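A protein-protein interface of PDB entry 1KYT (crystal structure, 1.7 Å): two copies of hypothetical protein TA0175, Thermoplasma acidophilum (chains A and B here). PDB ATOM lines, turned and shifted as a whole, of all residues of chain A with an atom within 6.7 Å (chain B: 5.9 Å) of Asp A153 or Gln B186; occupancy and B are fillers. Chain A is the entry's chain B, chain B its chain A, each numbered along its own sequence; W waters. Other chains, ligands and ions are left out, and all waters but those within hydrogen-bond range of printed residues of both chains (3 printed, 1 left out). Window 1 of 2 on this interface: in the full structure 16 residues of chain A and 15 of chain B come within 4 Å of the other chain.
The side-chain carboxylate of Asp A153 sits at hydrogen-bond distance from the backbone NH of Phe A156, at 3.0 Å.
NE2 of Gln B186 is in hydrogen-bond range of O of Pro B183, 2.7 Å away.
OD1 of Asp A153 lies within hydrogen-bond range of N of Ala A155 (3.0 Å).
NH1 of Arg A150 touches CG of Met B182, at 3.7 Å.
CB of Arg A150 touches CG1 of Val B204 (3.8 Å).
Gly A151 touches Gln B186.
Gln B186 touches Asp A153.
Phe A156 touches Pro B188.
Printed residues of chain B within 4 Å of Arg A150: Met B182 and Val B204.
Of the printed residues of chain B, Gly A151 touches Gln B186 (3.2 Å).
Asp A153 touches just one residue of chain B: Gln B186.
Of the printed residues of chain A, Gln B186 touches Gly A151 (3.2 Å) and Asp A153 (3.7 Å).
Printed residues of chain A within 4 Å of Pro B188: Phe A156 (3.6 Å).
Of the printed residues of chain A, Val B204 touches Arg A150 (3.8 Å).
The nearest printed residue of chain B that does not touch Arg A150 is Gln B186 (4.001 Å).
Of the 21 printed residues of chain A, 4 touch a printed residue of chain B.
Printed residues of chain A that touch a printed residue of chain B: Arg A150, Gly A151, Asp A153 and Phe A156.
Hydrophobic or aromatic side chains of chain A within 4 Å of the printed part of chain B: Phe A156.
Positions printed for both chains: 155, 183 and 184.
Of the 5 pairs that touch across the chains among the printed residues, none has its exchanged pair printed and touching as well.
Water W3 lies within hydrogen-bond range of the side-chain carboxylate of Asp A153 (2.5 Å) and the side-chain amide oxygen of Gln B186 (2.9 Å).
Water W1 bridges the side-chain amide oxygen (OE1) of Gln B186 (2.6 Å) and the side-chain carboxylate (OD1) of Asp A153 (2.7 Å).
Water W2 bridges the backbone carbonyl oxygen (O) of Gln B186 and the backbone carbonyl oxygen (O) of Gly A151.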
ATOM      1  N   LEU A  44     -32.852 -10.559  -9.738  1.00  0.00           N
ATOM      2  CA  LEU A  44     -31.776 -11.273 -10.397  1.00  0.00           C
ATOM      3  C   LEU A  44     -32.364 -12.309 -11.348  1.00  0.00           C
ATOM      4  O   LEU A  44     -33.396 -12.931 -11.052  1.00  0.00           O
ATOM      5  CB  LEU A  44     -30.895 -11.992  -9.382  1.00  0.00           C
ATOM      6  CG  LEU A  44     -30.366 -11.147  -8.226  1.00  0.00           C
ATOM      7  CD1 LEU A  44     -31.379 -11.130  -7.117  1.00  0.00           C
ATOM      8  CD2 LEU A  44     -29.058 -11.714  -7.740  1.00  0.00           C
ATOM      9  N   GLU A  68     -27.809 -11.864 -16.697  1.00  0.00           N
ATOM     10  CA  GLU A  68     -26.764 -12.854 -16.909  1.00  0.00           C
ATOM     11  C   GLU A  68     -26.337 -13.531 -15.607  1.00  0.00           C
ATOM     12  O   GLU A  68     -25.153 -13.638 -15.303  1.00  0.00           O
ATOM     13  CB  GLU A  68     -25.564 -12.193 -17.597  1.00  0.00           C
ATOM     14  CG  GLU A  68     -25.934 -11.496 -18.911  1.00  0.00           C
ATOM     15  CD  GLU A  68     -24.720 -10.996 -19.684  1.00  0.00           C
ATOM     16  OE1 GLU A  68     -23.765 -11.777 -19.881  1.00  0.00           O
ATOM     17  OE2 GLU A  68     -24.727  -9.818 -20.105  1.00  0.00           O
ATOM     18  N   ASN A  69     -27.330 -13.959 -14.835  1.00  0.00           N
ATOM     19  CA  ASN A  69     -27.118 -14.674 -13.579  1.00  0.00           C
ATOM     20  C   ASN A  69     -26.184 -14.037 -12.565  1.00  0.00           C
ATOM     21  O   ASN A  69     -25.549 -14.736 -11.789  1.00  0.00           O
ATOM     22  CB  ASN A  69     -26.635 -16.092 -13.869  1.00  0.00           C
ATOM     23  CG  ASN A  69     -27.558 -16.831 -14.799  1.00  0.00           C
ATOM     24  OD1 ASN A  69     -27.158 -17.234 -15.898  1.00  0.00           O
ATOM     25  ND2 ASN A  69     -28.810 -17.017 -14.366  1.00  0.00           N
ATOM     26  N   GLY A  70     -26.124 -12.712 -12.560  1.00  0.00           N
ATOM     27  CA  GLY A  70     -25.279 -12.017 -11.611  1.00  0.00           C
ATOM     28  C   GLY A  70     -24.061 -11.347 -12.216  1.00  0.00           C
ATOM     29  O   GLY A  70     -23.404 -10.571 -11.544  1.00  0.00           O
ATOM     30  N   GLY A  71     -23.783 -11.618 -13.485  1.00  0.00           N
ATOM     31  CA  GLY A  71     -22.599 -11.049 -14.123  1.00  0.00           C
ATOM     32  C   GLY A  71     -22.625  -9.590 -14.565  1.00  0.00           C
ATOM     33  O   GLY A  71     -21.579  -9.005 -14.840  1.00  0.00           O
ATOM     34  N   PHE A  84     -17.818  -9.544 -15.478  1.00  0.00           N
ATOM     35  CA  PHE A  84     -17.120 -10.559 -16.252  1.00  0.00           C
ATOM     36  C   PHE A  84     -17.245 -10.213 -17.729  1.00  0.00           C
ATOM     37  O   PHE A  84     -18.099  -9.421 -18.120  1.00  0.00           O
ATOM     38  CB  PHE A  84     -17.714 -11.948 -16.026  1.00  0.00           C
ATOM     39  CG  PHE A  84     -17.624 -12.417 -14.618  1.00  0.00           C
ATOM     40  CD1 PHE A  84     -18.508 -11.947 -13.664  1.00  0.00           C
ATOM     41  CD2 PHE A  84     -16.673 -13.363 -14.245  1.00  0.00           C
ATOM     42  CE1 PHE A  84     -18.458 -12.409 -12.351  1.00  0.00           C
ATOM     43  CE2 PHE A  84     -16.617 -13.832 -12.929  1.00  0.00           C
ATOM     44  CZ  PHE A  84     -17.516 -13.349 -11.986  1.00  0.00           C
ATOM     45  N   PHE A 139     -25.372 -24.639 -17.737  1.00  0.00           N
ATOM     46  CA  PHE A 139     -26.609 -25.092 -17.102  1.00  0.00           C
ATOM     47  C   PHE A 139     -27.739 -24.425 -17.844  1.00  0.00           C
ATOM     48  O   PHE A 139     -27.514 -23.489 -18.621  1.00  0.00           O
ATOM     49  CB  PHE A 139     -26.666 -24.718 -15.614  1.00  0.00           C
ATOM     50  CG  PHE A 139     -26.560 -23.252 -15.354  1.00  0.00           C
ATOM     51  CD1 PHE A 139     -27.660 -22.417 -15.525  1.00  0.00           C
ATOM     52  CD2 PHE A 139     -25.338 -22.695 -14.975  1.00  0.00           C
ATOM     53  CE1 PHE A 139     -27.543 -21.041 -15.329  1.00  0.00           C
ATOM     54  CE2 PHE A 139     -25.208 -21.331 -14.778  1.00  0.00           C
ATOM     55  CZ  PHE A 139     -26.317 -20.494 -14.954  1.00  0.00           C
ATOM     56  N   MET A 148     -21.352 -19.760 -18.522  1.00  0.00           N
ATOM     57  CA  MET A 148     -20.863 -18.783 -17.554  1.00  0.00           C
ATOM     58  C   MET A 148     -19.404 -18.983 -17.149  1.00  0.00           C
ATOM     59  O   MET A 148     -18.827 -20.041 -17.368  1.00  0.00           O
ATOM     60  CB  MET A 148     -21.694 -18.868 -16.275  1.00  0.00           C
ATOM     61  CG  MET A 148     -23.196 -18.958 -16.475  1.00  0.00           C
ATOM     62  SD  MET A 148     -23.927 -17.327 -17.218  1.00  0.00           S
ATOM     63  CE  MET A 148     -23.241 -16.107 -15.899  1.00  0.00           C
ATOM     64  N   ASN A 149     -18.810 -17.936 -16.581  1.00  0.00           N
ATOM     65  CA  ASN A 149     -17.461 -18.024 -16.049  1.00  0.00           C
ATOM     66  C   ASN A 149     -17.709 -18.610 -14.657  1.00  0.00           C
ATOM     67  O   ASN A 149     -18.746 -18.341 -14.053  1.00  0.00           O
ATOM     68  CB  ASN A 149     -16.835 -16.637 -15.919  1.00  0.00           C
ATOM     69  CG  ASN A 149     -16.628 -15.970 -17.250  1.00  0.00           C
ATOM     70  OD1 ASN A 149     -15.679 -16.276 -17.975  1.00  0.00           O
ATOM     71  ND2 ASN A 149     -17.529 -15.051 -17.593  1.00  0.00           N
ATOM     72  N   ARG A 150     -16.796 -19.440 -14.172  1.00  0.00           N
ATOM     73  CA  ARG A 150     -16.933 -20.045 -12.852  1.00  0.00           C
ATOM     74  C   ARG A 150     -17.011 -18.939 -11.803  1.00  0.00           C
ATOM     75  O   ARG A 150     -16.164 -18.054 -11.783  1.00  0.00           O
ATOM     76  CB  ARG A 150     -15.714 -20.928 -12.555  1.00  0.00           C
ATOM     77  CG  ARG A 150     -15.687 -21.533 -11.155  1.00  0.00           C
ATOM     78  CD  ARG A 150     -16.730 -22.640 -10.945  1.00  0.00           C
ATOM     79  NE  ARG A 150     -16.489 -23.812 -11.786  1.00  0.00           N
ATOM     80  CZ  ARG A 150     -16.945 -25.034 -11.520  1.00  0.00           C
ATOM     81  NH1 ARG A 150     -17.670 -25.268 -10.431  1.00  0.00           N
ATOM     82  NH2 ARG A 150     -16.675 -26.027 -12.348  1.00  0.00           N
ATOM     83  N   GLY A 151     -18.025 -18.997 -10.939  1.00  0.00           N
ATOM     84  CA  GLY A 151     -18.170 -17.999  -9.891  1.00  0.00           C
ATOM     85  C   GLY A 151     -19.048 -16.821 -10.275  1.00  0.00           C
ATOM     86  O   GLY A 151     -19.274 -15.901  -9.489  1.00  0.00           O
ATOM     87  N   GLU A 152     -19.540 -16.839 -11.504  1.00  0.00           N
ATOM     88  CA  GLU A 152     -20.401 -15.771 -11.974  1.00  0.00           C
ATOM     89  C   GLU A 152     -21.821 -16.209 -11.668  1.00  0.00           C
ATOM     90  O   GLU A 152     -22.515 -16.761 -12.528  1.00  0.00           O
ATOM     91  CB  GLU A 152     -20.215 -15.590 -13.468  1.00  0.00           C
ATOM     92  CG  GLU A 152     -21.094 -14.533 -14.080  1.00  0.00           C
ATOM     93  CD  GLU A 152     -20.619 -14.187 -15.473  1.00  0.00           C
ATOM     94  OE1 GLU A 152     -19.808 -14.973 -16.010  1.00  0.00           O
ATOM     95  OE2 GLU A 152     -21.049 -13.150 -16.026  1.00  0.00           O
ATOM     96  N   ASP A 153     -22.240 -16.002 -10.429  1.00  0.00           N
ATOM     97  CA  ASP A 153     -23.563 -16.430 -10.030  1.00  0.00           C
ATOM     98  C   ASP A 153     -24.301 -15.501  -9.076  1.00  0.00           C
ATOM     99  O   ASP A 153     -23.826 -14.425  -8.713  1.00  0.00           O
ATOM    100  CB  ASP A 153     -23.489 -17.850  -9.440  1.00  0.00           C
ATOM    101  CG  ASP A 153     -22.707 -17.913  -8.134  1.00  0.00           C
ATOM    102  OD1 ASP A 153     -22.408 -16.855  -7.545  1.00  0.00           O
ATOM    103  OD2 ASP A 153     -22.413 -19.039  -7.679  1.00  0.00           O
ATOM    104  N   LYS A 154     -25.472 -15.934  -8.652  1.00  0.00           N
ATOM    105  CA  LYS A 154     -26.263 -15.100  -7.788  1.00  0.00           C
ATOM    106  C   LYS A 154     -25.662 -14.859  -6.416  1.00  0.00           C
ATOM    107  O   LYS A 154     -26.031 -13.891  -5.749  1.00  0.00           O
ATOM    108  CB  LYS A 154     -27.667 -15.664  -7.688  1.00  0.00           C
ATOM    109  CG  LYS A 154     -28.359 -15.789  -9.030  1.00  0.00           C
ATOM    110  CD  LYS A 154     -29.867 -15.881  -8.813  1.00  0.00           C
ATOM    111  CE  LYS A 154     -30.628 -15.949 -10.106  1.00  0.00           C
ATOM    112  NZ  LYS A 154     -30.686 -17.340 -10.604  1.00  0.00           N
ATOM    113  N   ALA A 155     -24.744 -15.727  -5.985  1.00  0.00           N
ATOM    114  CA  ALA A 155     -24.084 -15.529  -4.684  1.00  0.00           C
ATOM    115  C   ALA A 155     -23.097 -14.372  -4.839  1.00  0.00           C
ATOM    116  O   ALA A 155     -22.874 -13.594  -3.914  1.00  0.00           O
ATOM    117  CB  ALA A 155     -23.339 -16.809  -4.243  1.00  0.00           C
ATOM    118  N   PHE A 156     -22.501 -14.273  -6.020  1.00  0.00           N
ATOM    119  CA  PHE A 156     -21.564 -13.200  -6.306  1.00  0.00           C
ATOM    120  C   PHE A 156     -22.366 -11.910  -6.235  1.00  0.00           C
ATOM    121  O   PHE A 156     -21.915 -10.921  -5.682  1.00  0.00           O
ATOM    122  CB  PHE A 156     -20.981 -13.339  -7.711  1.00  0.00           C
ATOM    123  CG  PHE A 156     -20.120 -12.182  -8.125  1.00  0.00           C
ATOM    124  CD1 PHE A 156     -18.775 -12.141  -7.787  1.00  0.00           C
ATOM    125  CD2 PHE A 156     -20.662 -11.114  -8.836  1.00  0.00           C
ATOM    126  CE1 PHE A 156     -17.980 -11.047  -8.153  1.00  0.00           C
ATOM    127  CE2 PHE A 156     -19.885 -10.036  -9.199  1.00  0.00           C
ATOM    128  CZ  PHE A 156     -18.536 -10.002  -8.857  1.00  0.00           C
ATOM    129  N   ALA A 157     -23.569 -11.940  -6.796  1.00  0.00           N
ATOM    130  CA  ALA A 157     -24.412 -10.754  -6.797  1.00  0.00           C
ATOM    131  C   ALA A 157     -24.872 -10.350  -5.401  1.00  0.00           C
ATOM    132  O   ALA A 157     -24.802  -9.180  -5.052  1.00  0.00           O
ATOM    133  CB  ALA A 157     -25.611 -10.961  -7.703  1.00  0.00           C
ATOM    134  N   VAL A 158     -25.330 -11.305  -4.598  1.00  0.00           N
ATOM    135  CA  VAL A 158     -25.819 -10.969  -3.269  1.00  0.00           C
ATOM    136  C   VAL A 158     -24.681 -10.420  -2.398  1.00  0.00           C
ATOM    137  O   VAL A 158     -24.873  -9.456  -1.674  1.00  0.00           O
ATOM    138  CB  VAL A 158     -26.551 -12.176  -2.606  1.00  0.00           C
ATOM    139  CG1 VAL A 158     -26.969 -11.833  -1.194  1.00  0.00           C
ATOM    140  CG2 VAL A 158     -27.821 -12.525  -3.418  1.00  0.00           C
ATOM    141  N   ASN A 180     -30.244 -23.282  -9.743  1.00  0.00           N
ATOM    142  CA  ASN A 180     -29.306 -22.192  -9.981  1.00  0.00           C
ATOM    143  C   ASN A 180     -29.538 -21.042  -9.011  1.00  0.00           C
ATOM    144  O   ASN A 180     -28.946 -19.977  -9.140  1.00  0.00           O
ATOM    145  CB  ASN A 180     -29.410 -21.680 -11.423  1.00  0.00           C
ATOM    146  CG  ASN A 180     -30.760 -21.090 -11.730  1.00  0.00           C
ATOM    147  OD1 ASN A 180     -30.896 -20.265 -12.632  1.00  0.00           O
ATOM    148  ND2 ASN A 180     -31.772 -21.508 -10.986  1.00  0.00           N
ATOM    149  N   PRO A 183     -27.075 -21.139  -4.871  1.00  0.00           N
ATOM    150  CA  PRO A 183     -25.935 -20.365  -4.384  1.00  0.00           C
ATOM    151  C   PRO A 183     -26.305 -19.277  -3.370  1.00  0.00           C
ATOM    152  O   PRO A 183     -25.568 -19.064  -2.423  1.00  0.00           O
ATOM    153  CB  PRO A 183     -25.334 -19.796  -5.667  1.00  0.00           C
ATOM    154  CG  PRO A 183     -25.600 -20.865  -6.656  1.00  0.00           C
ATOM    155  CD  PRO A 183     -27.040 -21.249  -6.340  1.00  0.00           C
ATOM    156  N   MET A 184     -27.440 -18.597  -3.552  1.00  0.00           N
ATOM    157  CA  MET A 184     -27.835 -17.558  -2.600  1.00  0.00           C
ATOM    158  C   MET A 184     -28.146 -18.197  -1.255  1.00  0.00           C
ATOM    159  O   MET A 184     -27.907 -17.600  -0.202  1.00  0.00           O
ATOM    160  CB  MET A 184     -29.099 -16.810  -3.057  1.00  0.00           C
ATOM    161  CG  MET A 184     -29.090 -16.322  -4.483  1.00  0.00           C
ATOM    162  SD  MET A 184     -30.449 -14.979  -4.782  1.00  0.00           S
ATOM    163  CE  MET A 184     -32.043 -16.069  -4.626  1.00  0.00           C
ATOM    164  N   ALA B 155     -15.938 -21.284   1.497  1.00  0.00           N
ATOM    165  CA  ALA B 155     -16.330 -19.973   0.973  1.00  0.00           C
ATOM    166  C   ALA B 155     -16.732 -19.117   2.177  1.00  0.00           C
ATOM    167  O   ALA B 155     -16.374 -17.942   2.280  1.00  0.00           O
ATOM    168  CB  ALA B 155     -17.502 -20.113   0.004  1.00  0.00           C
ATOM    169  N   ASP B 181     -12.846 -28.004  -2.358  1.00  0.00           N
ATOM    170  CA  ASP B 181     -12.220 -26.686  -2.244  1.00  0.00           C
ATOM    171  C   ASP B 181     -12.869 -25.734  -3.253  1.00  0.00           C
ATOM    172  O   ASP B 181     -12.586 -24.523  -3.252  1.00  0.00           O
ATOM    173  CB  ASP B 181     -10.731 -26.726  -2.560  1.00  0.00           C
ATOM    174  CG  ASP B 181      -9.974 -27.630  -1.650  1.00  0.00           C
ATOM    175  OD1 ASP B 181     -10.056 -27.437  -0.415  1.00  0.00           O
ATOM    176  OD2 ASP B 181      -9.292 -28.534  -2.183  1.00  0.00           O
ATOM    177  N   MET B 182     -13.733 -26.256  -4.117  1.00  0.00           N
ATOM    178  CA  MET B 182     -14.332 -25.384  -5.124  1.00  0.00           C
ATOM    179  C   MET B 182     -15.099 -24.210  -4.527  1.00  0.00           C
ATOM    180  O   MET B 182     -15.092 -23.121  -5.088  1.00  0.00           O
ATOM    181  CB  MET B 182     -15.211 -26.177  -6.101  1.00  0.00           C
ATOM    182  CG  MET B 182     -15.716 -25.346  -7.289  1.00  0.00           C
ATOM    183  SD  MET B 182     -14.345 -24.439  -8.368  1.00  0.00           S
ATOM    184  CE  MET B 182     -13.925 -25.903  -9.552  1.00  0.00           C
ATOM    185  N   PRO B 183     -15.779 -24.408  -3.385  1.00  0.00           N
ATOM    186  CA  PRO B 183     -16.497 -23.256  -2.832  1.00  0.00           C
ATOM    187  C   PRO B 183     -15.608 -22.009  -2.675  1.00  0.00           C
ATOM    188  O   PRO B 183     -16.064 -20.897  -2.918  1.00  0.00           O
ATOM    189  CB  PRO B 183     -17.016 -23.785  -1.495  1.00  0.00           C
ATOM    190  CG  PRO B 183     -17.316 -25.214  -1.818  1.00  0.00           C
ATOM    191  CD  PRO B 183     -16.088 -25.631  -2.623  1.00  0.00           C
ATOM    192  N   MET B 184     -14.347 -22.177  -2.287  1.00  0.00           N
ATOM    193  CA  MET B 184     -13.504 -21.005  -2.152  1.00  0.00           C
ATOM    194  C   MET B 184     -12.792 -20.664  -3.460  1.00  0.00           C
ATOM    195  O   MET B 184     -12.354 -19.537  -3.644  1.00  0.00           O
ATOM    196  CB  MET B 184     -12.497 -21.137  -0.986  1.00  0.00           C
ATOM    197  CG  MET B 184     -11.423 -22.210  -1.088  1.00  0.00           C
ATOM    198  SD  MET B 184     -10.142 -22.040   0.384  1.00  0.00           S
ATOM    199  CE  MET B 184      -9.050 -23.589  -0.018  1.00  0.00           C
ATOM    200  N   PHE B 185     -12.702 -21.608  -4.387  1.00  0.00           N
ATOM    201  CA  PHE B 185     -12.043 -21.279  -5.657  1.00  0.00           C
ATOM    202  C   PHE B 185     -12.984 -20.515  -6.593  1.00  0.00           C
ATOM    203  O   PHE B 185     -12.540 -19.801  -7.491  1.00  0.00           O
ATOM    204  CB  PHE B 185     -11.524 -22.540  -6.360  1.00  0.00           C
ATOM    205  CG  PHE B 185     -10.114 -22.897  -5.990  1.00  0.00           C
ATOM    206  CD1 PHE B 185      -9.802 -23.331  -4.697  1.00  0.00           C
ATOM    207  CD2 PHE B 185      -9.088 -22.740  -6.913  1.00  0.00           C
ATOM    208  CE1 PHE B 185      -8.489 -23.597  -4.332  1.00  0.00           C
ATOM    209  CE2 PHE B 185      -7.767 -23.007  -6.553  1.00  0.00           C
ATOM    210  CZ  PHE B 185      -7.469 -23.434  -5.259  1.00  0.00           C
ATOM    211  N   GLN B 186     -14.284 -20.658  -6.394  1.00  0.00           N
ATOM    212  CA  GLN B 186     -15.205 -19.951  -7.261  1.00  0.00           C
ATOM    213  C   GLN B 186     -15.371 -18.492  -6.844  1.00  0.00           C
ATOM    214  O   GLN B 186     -16.079 -17.735  -7.501  1.00  0.00           O
ATOM    215  CB  GLN B 186     -16.554 -20.685  -7.342  1.00  0.00           C
ATOM    216  CG  GLN B 186     -17.251 -20.986  -6.021  1.00  0.00           C
ATOM    217  CD  GLN B 186     -18.142 -19.848  -5.525  1.00  0.00           C
ATOM    218  OE1 GLN B 186     -19.050 -19.397  -6.230  1.00  0.00           O
ATOM    219  NE2 GLN B 186     -17.896 -19.396  -4.299  1.00  0.00           N
ATOM    220  N   LEU B 187     -14.714 -18.095  -5.753  1.00  0.00           N
ATOM    221  CA  LEU B 187     -14.756 -16.703  -5.303  1.00  0.00           C
ATOM    222  C   LEU B 187     -13.773 -15.905  -6.160  1.00  0.00           C
ATOM    223  O   LEU B 187     -12.902 -16.483  -6.801  1.00  0.00           O
ATOM    224  CB  LEU B 187     -14.363 -16.583  -3.826  1.00  0.00           C
ATOM    225  CG  LEU B 187     -15.276 -17.255  -2.804  1.00  0.00           C
ATOM    226  CD1 LEU B 187     -14.635 -17.182  -1.429  1.00  0.00           C
ATOM    227  CD2 LEU B 187     -16.637 -16.576  -2.801  1.00  0.00           C
ATOM    228  N   PRO B 188     -13.877 -14.562  -6.160  1.00  0.00           N
ATOM    229  CA  PRO B 188     -12.993 -13.705  -6.958  1.00  0.00           C
ATOM    230  C   PRO B 188     -11.593 -13.528  -6.390  1.00  0.00           C
ATOM    231  O   PRO B 188     -10.936 -12.516  -6.634  1.00  0.00           O
ATOM    232  CB  PRO B 188     -13.756 -12.371  -7.018  1.00  0.00           C
ATOM    233  CG  PRO B 188     -15.156 -12.723  -6.580  1.00  0.00           C
ATOM    234  CD  PRO B 188     -14.927 -13.754  -5.534  1.00  0.00           C
ATOM    235  N   LYS B 191      -5.930 -17.685  -6.998  1.00  0.00           N
ATOM    236  CA  LYS B 191      -5.915 -19.135  -6.826  1.00  0.00           C
ATOM    237  C   LYS B 191      -4.651 -19.842  -7.275  1.00  0.00           C
ATOM    238  O   LYS B 191      -4.067 -19.497  -8.307  1.00  0.00           O
ATOM    239  CB  LYS B 191      -7.086 -19.726  -7.609  1.00  0.00           C
ATOM    240  CG  LYS B 191      -8.446 -19.197  -7.220  1.00  0.00           C
ATOM    241  CD  LYS B 191      -9.479 -19.618  -8.248  1.00  0.00           C
ATOM    242  CE  LYS B 191     -10.102 -18.430  -8.918  1.00  0.00           C
ATOM    243  NZ  LYS B 191     -10.996 -17.724  -7.973  1.00  0.00           N
ATOM    244  N   VAL B 204      -9.371 -23.158 -13.222  1.00  0.00           N
ATOM    245  CA  VAL B 204      -9.653 -21.813 -12.725  1.00  0.00           C
ATOM    246  C   VAL B 204      -8.519 -21.204 -11.880  1.00  0.00           C
ATOM    247  O   VAL B 204      -8.628 -20.072 -11.416  1.00  0.00           O
ATOM    248  CB  VAL B 204     -10.970 -21.795 -11.895  1.00  0.00           C
ATOM    249  CG1 VAL B 204     -12.133 -22.255 -12.763  1.00  0.00           C
ATOM    250  CG2 VAL B 204     -10.844 -22.697 -10.679  1.00  0.00           C
HETATM  251  O   HOH W   1     -20.236 -17.136  -5.964  1.00  0.00           O
HETATM  252  O   HOH W   2     -16.984 -15.320  -7.943  1.00  0.00           O
HETATM  253  O   HOH W   3     -21.754 -20.119  -5.474  1.00  0.00           O
